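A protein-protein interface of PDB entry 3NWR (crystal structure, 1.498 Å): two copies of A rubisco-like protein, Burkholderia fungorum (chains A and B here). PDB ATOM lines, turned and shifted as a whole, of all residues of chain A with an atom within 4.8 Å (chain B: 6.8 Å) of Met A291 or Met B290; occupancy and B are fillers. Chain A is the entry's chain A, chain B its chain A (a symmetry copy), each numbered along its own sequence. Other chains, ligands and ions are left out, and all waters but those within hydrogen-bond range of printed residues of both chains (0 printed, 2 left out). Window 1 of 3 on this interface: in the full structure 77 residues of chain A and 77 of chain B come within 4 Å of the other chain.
Tyr A119 touches Gly B289, and with the chains exchanged Gly A289 touches Tyr B119. Tyr A119 touches Met B290, and with the chains exchanged Met A290 touches Tyr B119. Met A290 touches Met B291, and with the chains exchanged Met A291 touches Met B290. Met A290 touches Leu B297, and with the chains exchanged Leu A297 touches Met B290. Positions printed for both chains: 119, 263, 287, 288, 289, 290, 291, 292, 293, 297 and 298.
Of the printed residues of chain B, Leu A297 touches Met B290 (3.6 Å) and Asp B294 (3.9 Å). Gly B287 touches none of the printed residues of chain A. Met B290 touches just these residues of chain A: Tyr A119 (3.5 Å), Met A290 (3.8 Å), Met A291 (3.5 Å), Leu A297 (3.6 Å) and Gly A298 (3.7 Å). Ser B292 touches none of the printed residues of chain A. Printed residues of chain A within 4 Å of Arg B293: Tyr A119. The nearest residue of chain B that does not touch Met A291 is Trp B264 (4.8 Å).
The backbone carbonyl oxygen (O) of Gly A298 is in hydrogen-bond range of the side-chain hydroxyl (OH) of Tyr A119 (2.8 Å). OH of Tyr B119 is in hydrogen-bond range of O of Gly B298, 2.8 Å away. O of Met A291 is in hydrogen-bond range of N of Met A299, at 2.8 Å.
Of the 13 printed residues of chain A, 7 touch a printed residue of chain B. Hydrophobic or aromatic side chains of chain A that line the printed part of chain B: Tyr A119, Met A290, Met A291 and Leu A297. Along chain A the printed residues that touch a printed residue of chain B span positions 119 to 298. Of the 13 printed residues of chain B, 8 touch a printed residue of chain A. Printed residues of chain B that touch a printed residue of chain A: Tyr B119, Gly B289, Met B290, Met B291, Arg B293, Asp B294, Leu B297 and Gly B298. Hydrophobic or aromatic side chains of chain B within 4 Å of the printed part of chain A: Tyr B119, Met B290, Met B291 and Leu B297. Among the printed residues, no Asp or Glu carboxylate lies within 4 Å of a Lys or Arg side-chain nitrogen of the other chain.
Among the printed residues, pairs that only touch across the chains: Met A290 with Tyr B119, Tyr A119 with Met B290, Met A291 with Met B290, Met A290 with Met B291, Met A290 with Leu B297, Leu A297 with Met B290, Met A290 with Gly B298, Gly A298 with Met B290, Gly A289 with Tyr B119, Tyr A119 with Gly B289, Met A290 with Met B290 and Leu A297 with Asp B294.
The guanidinium group (NH1) of Arg A293 is in hydrogen-bond range of the backbone carbonyl oxygen (O) of Tyr B119, at 2.8 Å. NH1 of Arg B293 is in hydrogen-bond range of O of Tyr A119, at 2.8 Å.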
ATOM      1  N   TYR A 119      -8.043  29.986  15.265  1.00  0.00           N
ATOM      2  CA  TYR A 119      -8.323  30.975  14.240  1.00  0.00           C
ATOM      3  C   TYR A 119      -8.520  32.366  14.813  1.00  0.00           C
ATOM      4  O   TYR A 119      -8.389  33.349  14.093  1.00  0.00           O
ATOM      5  CB  TYR A 119      -9.547  30.567  13.414  1.00  0.00           C
ATOM      6  CG  TYR A 119      -9.336  29.244  12.723  1.00  0.00           C
ATOM      7  CD1 TYR A 119      -8.433  29.129  11.673  1.00  0.00           C
ATOM      8  CD2 TYR A 119      -9.997  28.111  13.154  1.00  0.00           C
ATOM      9  CE1 TYR A 119      -8.211  27.915  11.056  1.00  0.00           C
ATOM     10  CE2 TYR A 119      -9.800  26.898  12.536  1.00  0.00           C
ATOM     11  CZ  TYR A 119      -8.897  26.807  11.494  1.00  0.00           C
ATOM     12  OH  TYR A 119      -8.704  25.603  10.880  1.00  0.00           O
ATOM     13  N   ASN A 263     -21.052  19.332   6.568  1.00  0.00           N
ATOM     14  CA  ASN A 263     -20.687  20.468   7.405  1.00  0.00           C
ATOM     15  C   ASN A 263     -21.811  20.888   8.345  1.00  0.00           C
ATOM     16  O   ASN A 263     -21.566  21.283   9.482  1.00  0.00           O
ATOM     17  CB  ASN A 263     -20.246  21.653   6.561  1.00  0.00           C
ATOM     18  CG  ASN A 263     -18.996  21.355   5.780  1.00  0.00           C
ATOM     19  OD1 ASN A 263     -18.031  20.793   6.327  1.00  0.00           O
ATOM     20  ND2 ASN A 263     -19.002  21.695   4.494  1.00  0.00           N
ATOM     21  N   GLY A 287     -20.324  24.256   1.661  1.00  0.00           N
ATOM     22  CA  GLY A 287     -19.937  25.083   2.785  1.00  0.00           C
ATOM     23  C   GLY A 287     -18.429  25.044   2.983  1.00  0.00           C
ATOM     24  O   GLY A 287     -17.869  25.909   3.661  1.00  0.00           O
ATOM     25  N   TYR A 288     -17.770  24.048   2.395  1.00  0.00           N
ATOM     26  CA  TYR A 288     -16.321  23.923   2.546  1.00  0.00           C
ATOM     27  C   TYR A 288     -15.569  25.130   1.951  1.00  0.00           C
ATOM     28  O   TYR A 288     -14.473  25.465   2.403  1.00  0.00           O
ATOM     29  CB  TYR A 288     -15.799  22.584   1.982  1.00  0.00           C
ATOM     30  CG  TYR A 288     -14.291  22.499   2.012  1.00  0.00           C
ATOM     31  CD1 TYR A 288     -13.605  22.489   3.224  1.00  0.00           C
ATOM     32  CD2 TYR A 288     -13.553  22.455   0.841  1.00  0.00           C
ATOM     33  CE1 TYR A 288     -12.222  22.441   3.266  1.00  0.00           C
ATOM     34  CE2 TYR A 288     -12.158  22.398   0.870  1.00  0.00           C
ATOM     35  CZ  TYR A 288     -11.506  22.388   2.088  1.00  0.00           C
ATOM     36  OH  TYR A 288     -10.122  22.354   2.124  1.00  0.00           O
ATOM     37  N   GLY A 289     -16.168  25.807   0.974  1.00  0.00           N
ATOM     38  CA  GLY A 289     -15.571  27.020   0.428  1.00  0.00           C
ATOM     39  C   GLY A 289     -15.392  28.104   1.487  1.00  0.00           C
ATOM     40  O   GLY A 289     -14.399  28.838   1.496  1.00  0.00           O
ATOM     41  N   MET A 290     -16.365  28.233   2.378  1.00  0.00           N
ATOM     42  CA  MET A 290     -16.232  29.157   3.497  1.00  0.00           C
ATOM     43  C   MET A 290     -15.022  28.806   4.362  1.00  0.00           C
ATOM     44  O   MET A 290     -14.388  29.696   4.923  1.00  0.00           O
ATOM     45  CB  MET A 290     -17.506  29.151   4.349  1.00  0.00           C
ATOM     46  CG  MET A 290     -17.315  29.733   5.737  1.00  0.00           C
ATOM     47  SD  MET A 290     -18.864  29.866   6.660  1.00  0.00           S
ATOM     48  CE  MET A 290     -19.246  28.138   6.841  1.00  0.00           C
ATOM     49  N   MET A 291     -14.700  27.515   4.439  1.00  0.00           N
ATOM     50  CA  MET A 291     -13.630  27.038   5.304  1.00  0.00           C
ATOM     51  C   MET A 291     -12.263  27.036   4.632  1.00  0.00           C
ATOM     52  O   MET A 291     -11.275  26.643   5.258  1.00  0.00           O
ATOM     53  CB  MET A 291     -13.947  25.613   5.788  1.00  0.00           C
ATOM     54  CG  MET A 291     -15.296  25.514   6.451  1.00  0.00           C
ATOM     55  SD  MET A 291     -15.764  23.813   6.806  1.00  0.00           S
ATOM     56  CE  MET A 291     -14.348  23.228   7.734  1.00  0.00           C
ATOM     57  N   SER A 292     -12.183  27.473   3.373  1.00  0.00           N
ATOM     58  CA  SER A 292     -10.961  27.242   2.601  1.00  0.00           C
ATOM     59  C   SER A 292     -10.585  28.229   1.488  1.00  0.00           C
ATOM     60  O   SER A 292      -9.446  28.174   1.022  1.00  0.00           O
ATOM     61  CB  SER A 292     -10.992  25.827   2.000  1.00  0.00           C
ATOM     62  OG  SER A 292     -12.050  25.699   1.057  1.00  0.00           O
ATOM     63  N   ARG A 293     -11.502  29.092   1.039  1.00  0.00           N
ATOM     64  CA  ARG A 293     -11.215  29.957  -0.129  1.00  0.00           C
ATOM     65  C   ARG A 293     -10.078  30.934   0.122  1.00  0.00           C
ATOM     66  O   ARG A 293      -9.384  31.316  -0.817  1.00  0.00           O
ATOM     67  CB  ARG A 293     -12.432  30.788  -0.579  1.00  0.00           C
ATOM     68  CG  ARG A 293     -13.591  30.045  -1.237  1.00  0.00           C
ATOM     69  CD  ARG A 293     -13.571  29.972  -2.778  1.00  0.00           C
ATOM     70  NE  ARG A 293     -13.036  31.117  -3.537  1.00  0.00           N
ATOM     71  CZ  ARG A 293     -13.758  31.943  -4.299  1.00  0.00           C
ATOM     72  NH1 ARG A 293     -15.083  31.819  -4.391  1.00  0.00           N
ATOM     73  NH2 ARG A 293     -13.145  32.901  -4.981  1.00  0.00           N
ATOM     74  N   LEU A 297      -6.408  31.263   5.713  1.00  0.00           N
ATOM     75  CA  LEU A 297      -7.381  30.927   6.746  1.00  0.00           C
ATOM     76  C   LEU A 297      -7.992  29.555   6.537  1.00  0.00           C
ATOM     77  O   LEU A 297      -8.106  29.088   5.415  1.00  0.00           O
ATOM     78  CB  LEU A 297      -8.503  31.975   6.748  1.00  0.00           C
ATOM     79  CG  LEU A 297      -9.570  31.934   7.843  1.00  0.00           C
ATOM     80  CD1 LEU A 297      -8.931  32.137   9.217  1.00  0.00           C
ATOM     81  CD2 LEU A 297     -10.637  33.003   7.587  1.00  0.00           C
ATOM     82  N   GLY A 298      -8.394  28.922   7.632  1.00  0.00           N
ATOM     83  CA  GLY A 298      -9.272  27.768   7.544  1.00  0.00           C
ATOM     84  C   GLY A 298      -8.581  26.420   7.491  1.00  0.00           C
ATOM     85  O   GLY A 298      -7.707  26.134   8.308  1.00  0.00           O
ATOM     86  N   MET A 299      -8.959  25.597   6.518  1.00  0.00           N
ATOM     87  CA  MET A 299      -8.527  24.210   6.505  1.00  0.00           C
ATOM     88  C   MET A 299      -8.287  23.739   5.080  1.00  0.00           C
ATOM     89  O   MET A 299      -9.188  23.807   4.241  1.00  0.00           O
ATOM     90  CB  MET A 299      -9.598  23.342   7.171  1.00  0.00           C
ATOM     91  CG  MET A 299      -9.099  22.026   7.683  1.00  0.00           C
ATOM     92  SD  MET A 299     -10.442  21.133   8.506  1.00  0.00           S
ATOM     93  CE  MET A 299     -10.963  22.254   9.785  1.00  0.00           C
ATOM     94  N   TYR A 304      -9.110  18.465   6.321  1.00  0.00           N
ATOM     95  CA  TYR A 304     -10.567  18.376   6.285  1.00  0.00           C
ATOM     96  C   TYR A 304     -11.031  16.940   6.024  1.00  0.00           C
ATOM     97  O   TYR A 304     -11.880  16.397   6.751  1.00  0.00           O
ATOM     98  CB  TYR A 304     -11.076  19.303   5.181  1.00  0.00           C
ATOM     99  CG  TYR A 304     -12.578  19.367   4.997  1.00  0.00           C
ATOM    100  CD1 TYR A 304     -13.389  20.038   5.913  1.00  0.00           C
ATOM    101  CD2 TYR A 304     -13.177  18.795   3.875  1.00  0.00           C
ATOM    102  CE1 TYR A 304     -14.776  20.104   5.719  1.00  0.00           C
ATOM    103  CE2 TYR A 304     -14.549  18.865   3.673  1.00  0.00           C
ATOM    104  CZ  TYR A 304     -15.335  19.523   4.593  1.00  0.00           C
ATOM    105  OH  TYR A 304     -16.690  19.591   4.365  1.00  0.00           O
ATOM    106  N   TYR B 119     -20.202  29.940  -1.630  1.00  0.00           N
ATOM    107  CA  TYR B 119     -18.837  30.369  -1.390  1.00  0.00           C
ATOM    108  C   TYR B 119     -17.893  29.954  -2.503  1.00  0.00           C
ATOM    109  O   TYR B 119     -16.825  30.538  -2.650  1.00  0.00           O
ATOM    110  CB  TYR B 119     -18.330  29.839  -0.045  1.00  0.00           C
ATOM    111  CG  TYR B 119     -19.172  30.339   1.101  1.00  0.00           C
ATOM    112  CD1 TYR B 119     -19.138  31.677   1.475  1.00  0.00           C
ATOM    113  CD2 TYR B 119     -20.029  29.487   1.769  1.00  0.00           C
ATOM    114  CE1 TYR B 119     -19.929  32.148   2.503  1.00  0.00           C
ATOM    115  CE2 TYR B 119     -20.809  29.939   2.809  1.00  0.00           C
ATOM    116  CZ  TYR B 119     -20.761  31.273   3.162  1.00  0.00           C
ATOM    117  OH  TYR B 119     -21.533  31.720   4.195  1.00  0.00           O
ATOM    118  N   ASN B 263     -19.971  23.896  16.309  1.00  0.00           N
ATOM    119  CA  ASN B 263     -19.565  23.766  14.915  1.00  0.00           C
ATOM    120  C   ASN B 263     -19.218  22.331  14.537  1.00  0.00           C
ATOM    121  O   ASN B 263     -19.502  21.887  13.427  1.00  0.00           O
ATOM    122  CB  ASN B 263     -18.397  24.685  14.595  1.00  0.00           C
ATOM    123  CG  ASN B 263     -18.765  26.136  14.737  1.00  0.00           C
ATOM    124  OD1 ASN B 263     -19.832  26.564  14.264  1.00  0.00           O
ATOM    125  ND2 ASN B 263     -17.911  26.903  15.411  1.00  0.00           N
ATOM    126  N   TRP B 264     -18.615  21.613  15.477  1.00  0.00           N
ATOM    127  CA  TRP B 264     -18.135  20.271  15.189  1.00  0.00           C
ATOM    128  C   TRP B 264     -19.191  19.223  15.493  1.00  0.00           C
ATOM    129  O   TRP B 264     -19.194  18.137  14.905  1.00  0.00           O
ATOM    130  CB  TRP B 264     -16.851  20.012  15.982  1.00  0.00           C
ATOM    131  CG  TRP B 264     -15.890  21.167  15.914  1.00  0.00           C
ATOM    132  CD1 TRP B 264     -15.337  21.832  16.966  1.00  0.00           C
ATOM    133  CD2 TRP B 264     -15.399  21.811  14.728  1.00  0.00           C
ATOM    134  NE1 TRP B 264     -14.520  22.840  16.510  1.00  0.00           N
ATOM    135  CE2 TRP B 264     -14.538  22.848  15.143  1.00  0.00           C
ATOM    136  CE3 TRP B 264     -15.593  21.604  13.362  1.00  0.00           C
ATOM    137  CZ2 TRP B 264     -13.877  23.678  14.235  1.00  0.00           C
ATOM    138  CZ3 TRP B 264     -14.932  22.439  12.459  1.00  0.00           C
ATOM    139  CH2 TRP B 264     -14.083  23.448  12.906  1.00  0.00           C
ATOM    140  N   GLY B 287     -14.067  27.638  16.420  1.00  0.00           N
ATOM    141  CA  GLY B 287     -14.050  27.340  15.002  1.00  0.00           C
ATOM    142  C   GLY B 287     -14.744  28.442  14.216  1.00  0.00           C
ATOM    143  O   GLY B 287     -14.562  28.548  13.001  1.00  0.00           O
ATOM    144  N   TYR B 288     -15.538  29.262  14.901  1.00  0.00           N
ATOM    145  CA  TYR B 288     -16.258  30.338  14.224  1.00  0.00           C
ATOM    146  C   TYR B 288     -15.302  31.364  13.584  1.00  0.00           C
ATOM    147  O   TYR B 288     -15.651  32.006  12.591  1.00  0.00           O
ATOM    148  CB  TYR B 288     -17.288  31.014  15.156  1.00  0.00           C
ATOM    149  CG  TYR B 288     -17.945  32.212  14.509  1.00  0.00           C
ATOM    150  CD1 TYR B 288     -18.757  32.057  13.388  1.00  0.00           C
ATOM    151  CD2 TYR B 288     -17.737  33.492  14.997  1.00  0.00           C
ATOM    152  CE1 TYR B 288     -19.341  33.149  12.769  1.00  0.00           C
ATOM    153  CE2 TYR B 288     -18.328  34.600  14.385  1.00  0.00           C
ATOM    154  CZ  TYR B 288     -19.130  34.414  13.276  1.00  0.00           C
ATOM    155  OH  TYR B 288     -19.700  35.510  12.652  1.00  0.00           O
ATOM    156  N   GLY B 289     -14.089  31.490  14.116  1.00  0.00           N
ATOM    157  CA  GLY B 289     -13.091  32.361  13.509  1.00  0.00           C
ATOM    158  C   GLY B 289     -12.756  31.949  12.078  1.00  0.00           C
ATOM    159  O   GLY B 289     -12.544  32.789  11.198  1.00  0.00           O
ATOM    160  N   MET B 290     -12.680  30.647  11.835  1.00  0.00           N
ATOM    161  CA  MET B 290     -12.484  30.153  10.479  1.00  0.00           C
ATOM    162  C   MET B 290     -13.616  30.606   9.558  1.00  0.00           C
ATOM    163  O   MET B 290     -13.390  30.841   8.373  1.00  0.00           O
ATOM    164  CB  MET B 290     -12.385  28.624  10.476  1.00  0.00           C
ATOM    165  CG  MET B 290     -12.609  27.999   9.112  1.00  0.00           C
ATOM    166  SD  MET B 290     -12.324  26.214   9.104  1.00  0.00           S
ATOM    167  CE  MET B 290     -13.658  25.700  10.163  1.00  0.00           C
ATOM    168  N   MET B 291     -14.818  30.748  10.116  1.00  0.00           N
ATOM    169  CA  MET B 291     -15.999  31.080   9.332  1.00  0.00           C
ATOM    170  C   MET B 291     -16.220  32.579   9.175  1.00  0.00           C
ATOM    171  O   MET B 291     -17.195  32.989   8.539  1.00  0.00           O
ATOM    172  CB  MET B 291     -17.247  30.459   9.981  1.00  0.00           C
ATOM    173  CG  MET B 291     -17.111  28.974  10.193  1.00  0.00           C
ATOM    174  SD  MET B 291     -18.467  28.291  11.159  1.00  0.00           S
ATOM    175  CE  MET B 291     -19.895  28.859  10.239  1.00  0.00           C
ATOM    176  N   SER B 292     -15.334  33.405   9.735  1.00  0.00           N
ATOM    177  CA  SER B 292     -15.640  34.832   9.846  1.00  0.00           C
ATOM    178  C   SER B 292     -14.487  35.844   9.852  1.00  0.00           C
ATOM    179  O   SER B 292     -14.757  37.035   9.689  1.00  0.00           O
ATOM    180  CB  SER B 292     -16.504  35.078  11.093  1.00  0.00           C
ATOM    181  OG  SER B 292     -15.782  34.766  12.280  1.00  0.00           O
ATOM    182  N   ARG B 293     -13.238  35.414  10.061  1.00  0.00           N
ATOM    183  CA  ARG B 293     -12.125  36.379  10.216  1.00  0.00           C
ATOM    184  C   ARG B 293     -11.880  37.208   8.966  1.00  0.00           C
ATOM    185  O   ARG B 293     -11.415  38.341   9.066  1.00  0.00           O
ATOM    186  CB  ARG B 293     -10.788  35.705  10.579  1.00  0.00           C
ATOM    187  CG  ARG B 293     -10.653  35.110  11.978  1.00  0.00           C
ATOM    188  CD  ARG B 293     -10.030  36.024  13.053  1.00  0.00           C
ATOM    189  NE  ARG B 293      -8.967  36.967  12.657  1.00  0.00           N
ATOM    190  CZ  ARG B 293      -7.683  36.875  13.012  1.00  0.00           C
ATOM    191  NH1 ARG B 293      -7.237  35.850  13.740  1.00  0.00           N
ATOM    192  NH2 ARG B 293      -6.836  37.825  12.639  1.00  0.00           N
ATOM    193  N   ASP B 294     -12.139  36.641   7.794  1.00  0.00           N
ATOM    194  CA  ASP B 294     -11.952  37.376   6.540  1.00  0.00           C
ATOM    195  C   ASP B 294     -13.255  38.094   6.196  1.00  0.00           C
ATOM    196  O   ASP B 294     -14.267  37.442   5.938  1.00  0.00           O
ATOM    197  CB  ASP B 294     -11.549  36.404   5.426  1.00  0.00           C
ATOM    198  CG  ASP B 294     -11.328  37.087   4.091  1.00  0.00           C
ATOM    199  OD1 ASP B 294     -11.832  38.212   3.892  1.00  0.00           O
ATOM    200  OD2 ASP B 294     -10.653  36.466   3.235  1.00  0.00           O
ATOM    201  N   LEU B 297     -15.515  36.924   3.349  1.00  0.00           N
ATOM    202  CA  LEU B 297     -15.880  35.514   3.283  1.00  0.00           C
ATOM    203  C   LEU B 297     -16.663  35.063   4.500  1.00  0.00           C
ATOM    204  O   LEU B 297     -16.495  35.600   5.584  1.00  0.00           O
ATOM    205  CB  LEU B 297     -14.605  34.665   3.171  1.00  0.00           C
ATOM    206  CG  LEU B 297     -14.721  33.158   2.932  1.00  0.00           C
ATOM    207  CD1 LEU B 297     -15.416  32.883   1.598  1.00  0.00           C
ATOM    208  CD2 LEU B 297     -13.336  32.506   2.958  1.00  0.00           C
ATOM    209  N   GLY B 298     -17.512  34.061   4.311  1.00  0.00           N
ATOM    210  CA  GLY B 298     -18.071  33.336   5.439  1.00  0.00           C
ATOM    211  C   GLY B 298     -19.402  33.849   5.954  1.00  0.00           C
ATOM    212  O   GLY B 298     -20.332  34.062   5.178  1.00  0.00           O
